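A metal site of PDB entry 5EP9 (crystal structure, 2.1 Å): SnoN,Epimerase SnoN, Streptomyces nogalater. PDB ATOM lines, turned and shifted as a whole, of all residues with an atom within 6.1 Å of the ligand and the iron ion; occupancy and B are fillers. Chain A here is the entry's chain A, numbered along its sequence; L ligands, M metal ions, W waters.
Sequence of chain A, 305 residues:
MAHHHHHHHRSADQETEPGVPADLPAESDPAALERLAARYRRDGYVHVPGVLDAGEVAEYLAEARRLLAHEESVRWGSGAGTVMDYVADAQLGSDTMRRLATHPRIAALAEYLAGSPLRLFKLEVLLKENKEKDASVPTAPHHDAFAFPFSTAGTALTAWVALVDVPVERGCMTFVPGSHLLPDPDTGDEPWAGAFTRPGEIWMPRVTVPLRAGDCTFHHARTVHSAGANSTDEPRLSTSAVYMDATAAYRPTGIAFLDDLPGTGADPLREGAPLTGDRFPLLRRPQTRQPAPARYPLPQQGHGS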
ATOM      1  N   TRP A  76      30.971  -2.140  11.012  1.00  0.00           N
ATOM      2  CA  TRP A  76      31.210  -2.623  12.362  1.00  0.00           C
ATOM      3  C   TRP A  76      32.501  -3.461  12.381  1.00  0.00           C
ATOM      4  O   TRP A  76      32.572  -4.606  11.924  1.00  0.00           O
ATOM      5  CB  TRP A  76      30.037  -3.450  12.888  1.00  0.00           C
ATOM      6  CG  TRP A  76      30.138  -3.963  14.359  1.00  0.00           C
ATOM      7  CD1 TRP A  76      31.135  -3.708  15.264  1.00  0.00           C
ATOM      8  CD2 TRP A  76      29.186  -4.802  15.048  1.00  0.00           C
ATOM      9  NE1 TRP A  76      30.854  -4.339  16.461  1.00  0.00           N
ATOM     10  CE2 TRP A  76      29.671  -5.016  16.359  1.00  0.00           C
ATOM     11  CE3 TRP A  76      27.966  -5.365  14.697  1.00  0.00           C
ATOM     12  CZ2 TRP A  76      28.975  -5.815  17.303  1.00  0.00           C
ATOM     13  CZ3 TRP A  76      27.232  -6.152  15.630  1.00  0.00           C
ATOM     14  CH2 TRP A  76      27.747  -6.377  16.922  1.00  0.00           C
ATOM     15  N   VAL A  83      33.454  -7.314  11.494  1.00  0.00           N
ATOM     16  CA  VAL A  83      32.334  -8.013  12.059  1.00  0.00           C
ATOM     17  C   VAL A  83      31.240  -8.038  11.022  1.00  0.00           C
ATOM     18  O   VAL A  83      30.637  -9.080  10.764  1.00  0.00           O
ATOM     19  CB  VAL A  83      31.837  -7.348  13.367  1.00  0.00           C
ATOM     20  CG1 VAL A  83      30.681  -8.107  13.907  1.00  0.00           C
ATOM     21  CG2 VAL A  83      32.951  -7.295  14.462  1.00  0.00           C
ATOM     22  N   MET A  84      30.956  -6.881  10.464  1.00  0.00           N
ATOM     23  CA  MET A  84      29.941  -6.740   9.430  1.00  0.00           C
ATOM     24  C   MET A  84      29.922  -5.353   8.786  1.00  0.00           C
ATOM     25  O   MET A  84      30.443  -4.406   9.338  1.00  0.00           O
ATOM     26  CB  MET A  84      28.520  -7.001   9.946  1.00  0.00           C
ATOM     27  CG  MET A  84      28.079  -6.035  11.031  1.00  0.00           C
ATOM     28  SD  MET A  84      26.331  -6.455  11.406  1.00  0.00           S
ATOM     29  CE  MET A  84      26.510  -8.028  12.257  1.00  0.00           C
ATOM     30  N   LEU A 126      22.128  -6.447   6.863  1.00  0.00           N
ATOM     31  CA  LEU A 126      23.408  -6.940   7.369  1.00  0.00           C
ATOM     32  C   LEU A 126      24.135  -7.730   6.321  1.00  0.00           C
ATOM     33  O   LEU A 126      23.545  -8.542   5.663  1.00  0.00           O
ATOM     34  CB  LEU A 126      23.269  -7.782   8.631  1.00  0.00           C
ATOM     35  CG  LEU A 126      22.389  -7.196   9.726  1.00  0.00           C
ATOM     36  CD1 LEU A 126      22.323  -8.162  10.896  1.00  0.00           C
ATOM     37  CD2 LEU A 126      22.916  -5.880  10.209  1.00  0.00           C
ATOM     38  N   LYS A 128      27.851  -9.966   6.013  1.00  0.00           N
ATOM     39  CA  LYS A 128      29.161 -10.539   6.300  1.00  0.00           C
ATOM     40  C   LYS A 128      29.702 -11.218   5.117  1.00  0.00           C
ATOM     41  O   LYS A 128      29.092 -12.078   4.535  1.00  0.00           O
ATOM     42  CB  LYS A 128      29.147 -11.633   7.389  1.00  0.00           C
ATOM     43  CG  LYS A 128      28.975 -11.194   8.770  1.00  0.00           C
ATOM     44  CD  LYS A 128      29.303 -12.422   9.681  1.00  0.00           C
ATOM     45  CE  LYS A 128      28.924 -12.131  11.120  1.00  0.00           C
ATOM     46  NZ  LYS A 128      30.048 -11.594  11.913  1.00  0.00           N
ATOM     47  N   THR A 139      30.680 -12.343  15.100  1.00  0.00           N
ATOM     48  CA  THR A 139      30.004 -11.404  15.946  1.00  0.00           C
ATOM     49  C   THR A 139      30.128 -11.920  17.404  1.00  0.00           C
ATOM     50  O   THR A 139      29.546 -12.930  17.712  1.00  0.00           O
ATOM     51  CB  THR A 139      28.500 -11.310  15.577  1.00  0.00           C
ATOM     52  OG1 THR A 139      28.373 -10.905  14.224  1.00  0.00           O
ATOM     53  CG2 THR A 139      27.873 -10.192  16.399  1.00  0.00           C
ATOM     54  N   HIS A 142      26.726 -11.131  22.941  1.00  0.00           N
ATOM     55  CA  HIS A 142      26.204  -9.988  23.598  1.00  0.00           C
ATOM     56  C   HIS A 142      24.724 -10.197  23.797  1.00  0.00           C
ATOM     57  O   HIS A 142      24.122 -11.097  23.222  1.00  0.00           O
ATOM     58  CB  HIS A 142      26.483  -8.749  22.761  1.00  0.00           C
ATOM     59  CG  HIS A 142      25.755  -8.758  21.443  1.00  0.00           C
ATOM     60  ND1 HIS A 142      26.176  -9.505  20.394  1.00  0.00           N
ATOM     61  CD2 HIS A 142      24.595  -8.198  21.050  1.00  0.00           C
ATOM     62  CE1 HIS A 142      25.349  -9.368  19.378  1.00  0.00           C
ATOM     63  NE2 HIS A 142      24.413  -8.529  19.726  1.00  0.00           N
ATOM     64  N   HIS A 143      24.124  -9.306  24.541  1.00  0.00           N
ATOM     65  CA  HIS A 143      22.671  -9.094  24.467  1.00  0.00           C
ATOM     66  C   HIS A 143      22.325  -7.712  24.041  1.00  0.00           C
ATOM     67  O   HIS A 143      23.130  -6.863  24.104  1.00  0.00           O
ATOM     68  CB  HIS A 143      21.902  -9.484  25.705  1.00  0.00           C
ATOM     69  CG  HIS A 143      22.253  -8.730  26.905  1.00  0.00           C
ATOM     70  ND1 HIS A 143      23.364  -9.026  27.649  1.00  0.00           N
ATOM     71  CD2 HIS A 143      21.595  -7.747  27.557  1.00  0.00           C
ATOM     72  CE1 HIS A 143      23.360  -8.273  28.729  1.00  0.00           C
ATOM     73  NE2 HIS A 143      22.285  -7.484  28.697  1.00  0.00           N
ATOM     74  N   ASP A 144      21.138  -7.517  23.503  1.00  0.00           N
ATOM     75  CA  ASP A 144      20.931  -6.285  22.718  1.00  0.00           C
ATOM     76  C   ASP A 144      20.424  -5.128  23.573  1.00  0.00           C
ATOM     77  O   ASP A 144      20.624  -3.968  23.234  1.00  0.00           O
ATOM     78  CB  ASP A 144      19.889  -6.549  21.562  1.00  0.00           C
ATOM     79  CG  ASP A 144      20.330  -7.504  20.563  1.00  0.00           C
ATOM     80  OD1 ASP A 144      21.529  -7.504  20.157  1.00  0.00           O
ATOM     81  OD2 ASP A 144      19.419  -8.199  20.064  1.00  0.00           O
ATOM     82  N   THR A 158      13.999  -8.879  18.355  1.00  0.00           N
ATOM     83  CA  THR A 158      14.618  -8.711  17.073  1.00  0.00           C
ATOM     84  C   THR A 158      14.226  -9.866  16.101  1.00  0.00           C
ATOM     85  O   THR A 158      14.340 -10.992  16.452  1.00  0.00           O
ATOM     86  CB  THR A 158      16.116  -8.603  17.231  1.00  0.00           C
ATOM     87  OG1 THR A 158      16.442  -7.449  18.001  1.00  0.00           O
ATOM     88  CG2 THR A 158      16.816  -8.565  15.875  1.00  0.00           C
ATOM     89  N   TRP A 160      15.392 -11.584  12.698  1.00  0.00           N
ATOM     90  CA  TRP A 160      16.562 -11.681  11.840  1.00  0.00           C
ATOM     91  C   TRP A 160      16.157 -12.581  10.690  1.00  0.00           C
ATOM     92  O   TRP A 160      15.858 -13.761  10.886  1.00  0.00           O
ATOM     93  CB  TRP A 160      17.720 -12.287  12.631  1.00  0.00           C
ATOM     94  CG  TRP A 160      19.137 -12.203  12.117  1.00  0.00           C
ATOM     95  CD1 TRP A 160      20.121 -11.390  12.604  1.00  0.00           C
ATOM     96  CD2 TRP A 160      19.741 -13.030  11.133  1.00  0.00           C
ATOM     97  NE1 TRP A 160      21.298 -11.655  11.969  1.00  0.00           N
ATOM     98  CE2 TRP A 160      21.075 -12.593  11.005  1.00  0.00           C
ATOM     99  CE3 TRP A 160      19.225 -13.974  10.215  1.00  0.00           C
ATOM    100  CZ2 TRP A 160      21.959 -13.175  10.133  1.00  0.00           C
ATOM    101  CZ3 TRP A 160      20.129 -14.571   9.281  1.00  0.00           C
ATOM    102  CH2 TRP A 160      21.489 -14.174   9.279  1.00  0.00           C
ATOM    103  N   GLY A 171      28.044 -18.077   8.783  1.00  0.00           N
ATOM    104  CA  GLY A 171      27.919 -17.162   9.933  1.00  0.00           C
ATOM    105  C   GLY A 171      26.572 -17.090  10.582  1.00  0.00           C
ATOM    106  O   GLY A 171      26.082 -15.981  10.869  1.00  0.00           O
ATOM    107  N   MET A 173      23.686 -17.618  13.449  1.00  0.00           N
ATOM    108  CA  MET A 173      23.682 -17.224  14.891  1.00  0.00           C
ATOM    109  C   MET A 173      23.680 -18.413  15.847  1.00  0.00           C
ATOM    110  O   MET A 173      23.192 -19.479  15.509  1.00  0.00           O
ATOM    111  CB  MET A 173      22.540 -16.264  15.212  1.00  0.00           C
ATOM    112  CG  MET A 173      22.699 -14.939  14.419  1.00  0.00           C
ATOM    113  SD  MET A 173      22.080 -13.469  15.284  1.00  0.00           S
ATOM    114  CE  MET A 173      20.453 -13.798  14.813  1.00  0.00           C
ATOM    115  N   HIS A 219      14.584 -13.112  18.487  1.00  0.00           N
ATOM    116  CA  HIS A 219      15.224 -13.188  19.811  1.00  0.00           C
ATOM    117  C   HIS A 219      14.924 -12.000  20.708  1.00  0.00           C
ATOM    118  O   HIS A 219      14.961 -10.819  20.308  1.00  0.00           O
ATOM    119  CB  HIS A 219      16.726 -13.508  19.705  1.00  0.00           C
ATOM    120  CG  HIS A 219      17.560 -12.405  19.202  1.00  0.00           C
ATOM    121  ND1 HIS A 219      17.792 -12.212  17.850  1.00  0.00           N
ATOM    122  CD2 HIS A 219      18.301 -11.478  19.843  1.00  0.00           C
ATOM    123  CE1 HIS A 219      18.649 -11.219  17.699  1.00  0.00           C
ATOM    124  NE2 HIS A 219      18.953 -10.746  18.876  1.00  0.00           N
ATOM    125  N   HIS A 225      23.548 -13.881  22.399  1.00  0.00           N
ATOM    126  CA  HIS A 225      23.669 -14.386  21.070  1.00  0.00           C
ATOM    127  C   HIS A 225      24.958 -13.909  20.449  1.00  0.00           C
ATOM    128  O   HIS A 225      25.573 -12.936  20.842  1.00  0.00           O
ATOM    129  CB  HIS A 225      22.494 -14.049  20.162  1.00  0.00           C
ATOM    130  CG  HIS A 225      22.220 -12.560  20.028  1.00  0.00           C
ATOM    131  ND1 HIS A 225      21.711 -11.852  21.075  1.00  0.00           N
ATOM    132  CD2 HIS A 225      22.455 -11.681  19.046  1.00  0.00           C
ATOM    133  CE1 HIS A 225      21.660 -10.572  20.731  1.00  0.00           C
ATOM    134  NE2 HIS A 225      22.038 -10.449  19.478  1.00  0.00           N
ATOM    135  N   SER A 226      25.387 -14.689  19.478  1.00  0.00           N
ATOM    136  CA  SER A 226      26.594 -14.416  18.725  1.00  0.00           C
ATOM    137  C   SER A 226      26.411 -14.926  17.307  1.00  0.00           C
ATOM    138  O   SER A 226      25.389 -15.504  16.977  1.00  0.00           O
ATOM    139  CB  SER A 226      27.789 -15.164  19.379  1.00  0.00           C
ATOM    140  OG  SER A 226      27.676 -16.530  19.191  1.00  0.00           O
ATOM    141  N   ALA A 227      27.458 -14.833  16.495  1.00  0.00           N
ATOM    142  CA  ALA A 227      27.400 -15.360  15.158  1.00  0.00           C
ATOM    143  C   ALA A 227      28.773 -15.685  14.694  1.00  0.00           C
ATOM    144  O   ALA A 227      29.764 -15.004  15.063  1.00  0.00           O
ATOM    145  CB  ALA A 227      26.730 -14.352  14.163  1.00  0.00           C
ATOM    146  N   GLY A 228      28.834 -16.673  13.824  1.00  0.00           N
ATOM    147  CA  GLY A 228      30.155 -17.093  13.273  1.00  0.00           C
ATOM    148  C   GLY A 228      30.656 -16.105  12.246  1.00  0.00           C
ATOM    149  O   GLY A 228      29.945 -15.204  11.767  1.00  0.00           O
ATOM    150  N   ARG A 236      26.906 -13.396   3.295  1.00  0.00           N
ATOM    151  CA  ARG A 236      25.805 -13.617   4.210  1.00  0.00           C
ATOM    152  C   ARG A 236      24.955 -12.308   4.165  1.00  0.00           C
ATOM    153  O   ARG A 236      25.444 -11.236   4.516  1.00  0.00           O
ATOM    154  CB  ARG A 236      26.277 -13.844   5.630  1.00  0.00           C
ATOM    155  CG  ARG A 236      25.160 -14.373   6.510  1.00  0.00           C
ATOM    156  CD  ARG A 236      25.478 -14.207   7.965  1.00  0.00           C
ATOM    157  NE  ARG A 236      25.317 -12.837   8.404  1.00  0.00           N
ATOM    158  CZ  ARG A 236      25.477 -12.393   9.636  1.00  0.00           C
ATOM    159  NH1 ARG A 236      25.932 -13.142  10.629  1.00  0.00           N
ATOM    160  NH2 ARG A 236      25.266 -11.125   9.878  1.00  0.00           N
ATOM    161  N   SER A 238      21.093 -10.547   5.168  1.00  0.00           N
ATOM    162  CA  SER A 238      19.933 -10.696   6.021  1.00  0.00           C
ATOM    163  C   SER A 238      19.473  -9.341   6.411  1.00  0.00           C
ATOM    164  O   SER A 238      20.205  -8.333   6.224  1.00  0.00           O
ATOM    165  CB  SER A 238      20.296 -11.508   7.313  1.00  0.00           C
ATOM    166  OG  SER A 238      21.354 -10.880   8.029  1.00  0.00           O
ATOM    167  N   SER A 240      17.800  -7.342   9.998  1.00  0.00           N
ATOM    168  CA  SER A 240      17.526  -7.371  11.428  1.00  0.00           C
ATOM    169  C   SER A 240      16.686  -6.199  11.849  1.00  0.00           C
ATOM    170  O   SER A 240      17.053  -5.057  11.652  1.00  0.00           O
ATOM    171  CB  SER A 240      18.872  -7.398  12.185  1.00  0.00           C
ATOM    172  OG  SER A 240      18.679  -7.689  13.496  1.00  0.00           O
HETATM  173  C1  LIG L   1      21.205  -8.969  16.360  1.00  0.00           C
HETATM  174  O1  LIG L   1      20.815  -8.540  17.474  1.00  0.00           O
HETATM  175  O2  LIG L   1      20.413  -9.141  15.398  1.00  0.00           O
HETATM  176  C2  LIG L   1      22.621  -9.371  16.177  1.00  0.00           C
HETATM  177  O3  LIG L   1      23.419  -9.227  17.127  1.00  0.00           O
HETATM  178  C3  LIG L   1      23.038  -9.911  14.788  1.00  0.00           C
HETATM  179  C4  LIG L   1      24.442 -10.474  14.675  1.00  0.00           C
HETATM  180  C5  LIG L   1      24.861 -10.975  13.309  1.00  0.00           C
HETATM  181  O4  LIG L   1      24.022 -10.989  12.390  1.00  0.00           O
HETATM  182  O5  LIG L   1      26.057 -11.334  13.103  1.00  0.00           O
HETATM  183 FE    FE M   1      22.499  -8.530  18.692  1.00  0.00          FE
HETATM  184  O   HOH W   1      23.029  -6.621  15.238  1.00  0.00           O
HETATM  185  O   HOH W   2      23.007  -6.720  17.808  1.00  0.00           O
HETATM  186  O   HOH W   3      18.908  -6.568  17.629  1.00  0.00           O
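NE2 of His 225 lies close to NE2 of His 219 (3.2 Å).
N of Thr 139 lies within hydrogen-bond range of O of Ala 227.
The side-chain hydroxyl of Thr 139 sits at hydrogen-bond distance from the side-chain amino group of Lys 128, at 2.9 Å.
N of Arg 236 sits at hydrogen-bond distance from O of Lys 128 (2.8 Å).
O of His 219 sits at hydrogen-bond distance from N of Thr 158 (2.9 Å).
The backbone carbonyl oxygen of Met 84 is in hydrogen-bond range of the backbone NH of Trp 76 (2.9 Å).
O of Val 83 is in hydrogen-bond range of NZ of Lys 128 (2.8 Å).
The backbone NH (N) of Leu 126 is in hydrogen-bond range of the backbone carbonyl oxygen (O) of Ser 238 (2.8 Å).
CE of Met 84 touches O5 of the ligand (3.4 Å).
CD1 of Leu 126 touches O4 of the ligand (3.6 Å).
CE of Lys 128 touches O5 of the ligand, 3.6 Å away.
CG2 of Thr 158 touches O2 of the ligand, at 3.7 Å.
SD of Met 173 touches C3 of the ligand, 3.7 Å away.
CB of Ala 227 touches O5 of the ligand, at 3.3 Å.
Water W3 lies within hydrogen-bond range of the side-chain hydroxyl of Thr 158 and the side-chain carboxylate of Asp 144.
The iron ion is bound by an oxygen (O3) of the ligand, the side-chain carboxylate of Asp 144, water W2, an oxygen (O1) of the ligand, a ring nitrogen (NE2) of His 225 and a ring nitrogen (NE2) of His 142.
The iron ion has six donor atoms within binding distance.
Of the 21 residues printed, 3 come within 4 Å of the iron ion.
The nearest printed residue that does not touch the iron ion is His 219 (4.2 Å).
O5 of the ligand sits at hydrogen-bond distance from OG1 of Thr 139.
The guanidinium group (NH2) of Arg 236 lies within salt-bridge range of an oxygen (O4) of the ligand (2.8 Å).
An oxygen (O4) of the ligand sits at hydrogen-bond distance from the indole nitrogen (NE1) of Trp 160 (2.8 Å).
OG of Ser 240 lies within hydrogen-bond range of O2 of the ligand, 3.0 Å away.
NE2 of His 219 sits close to O1 of the ligand, 3.2 Å away.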
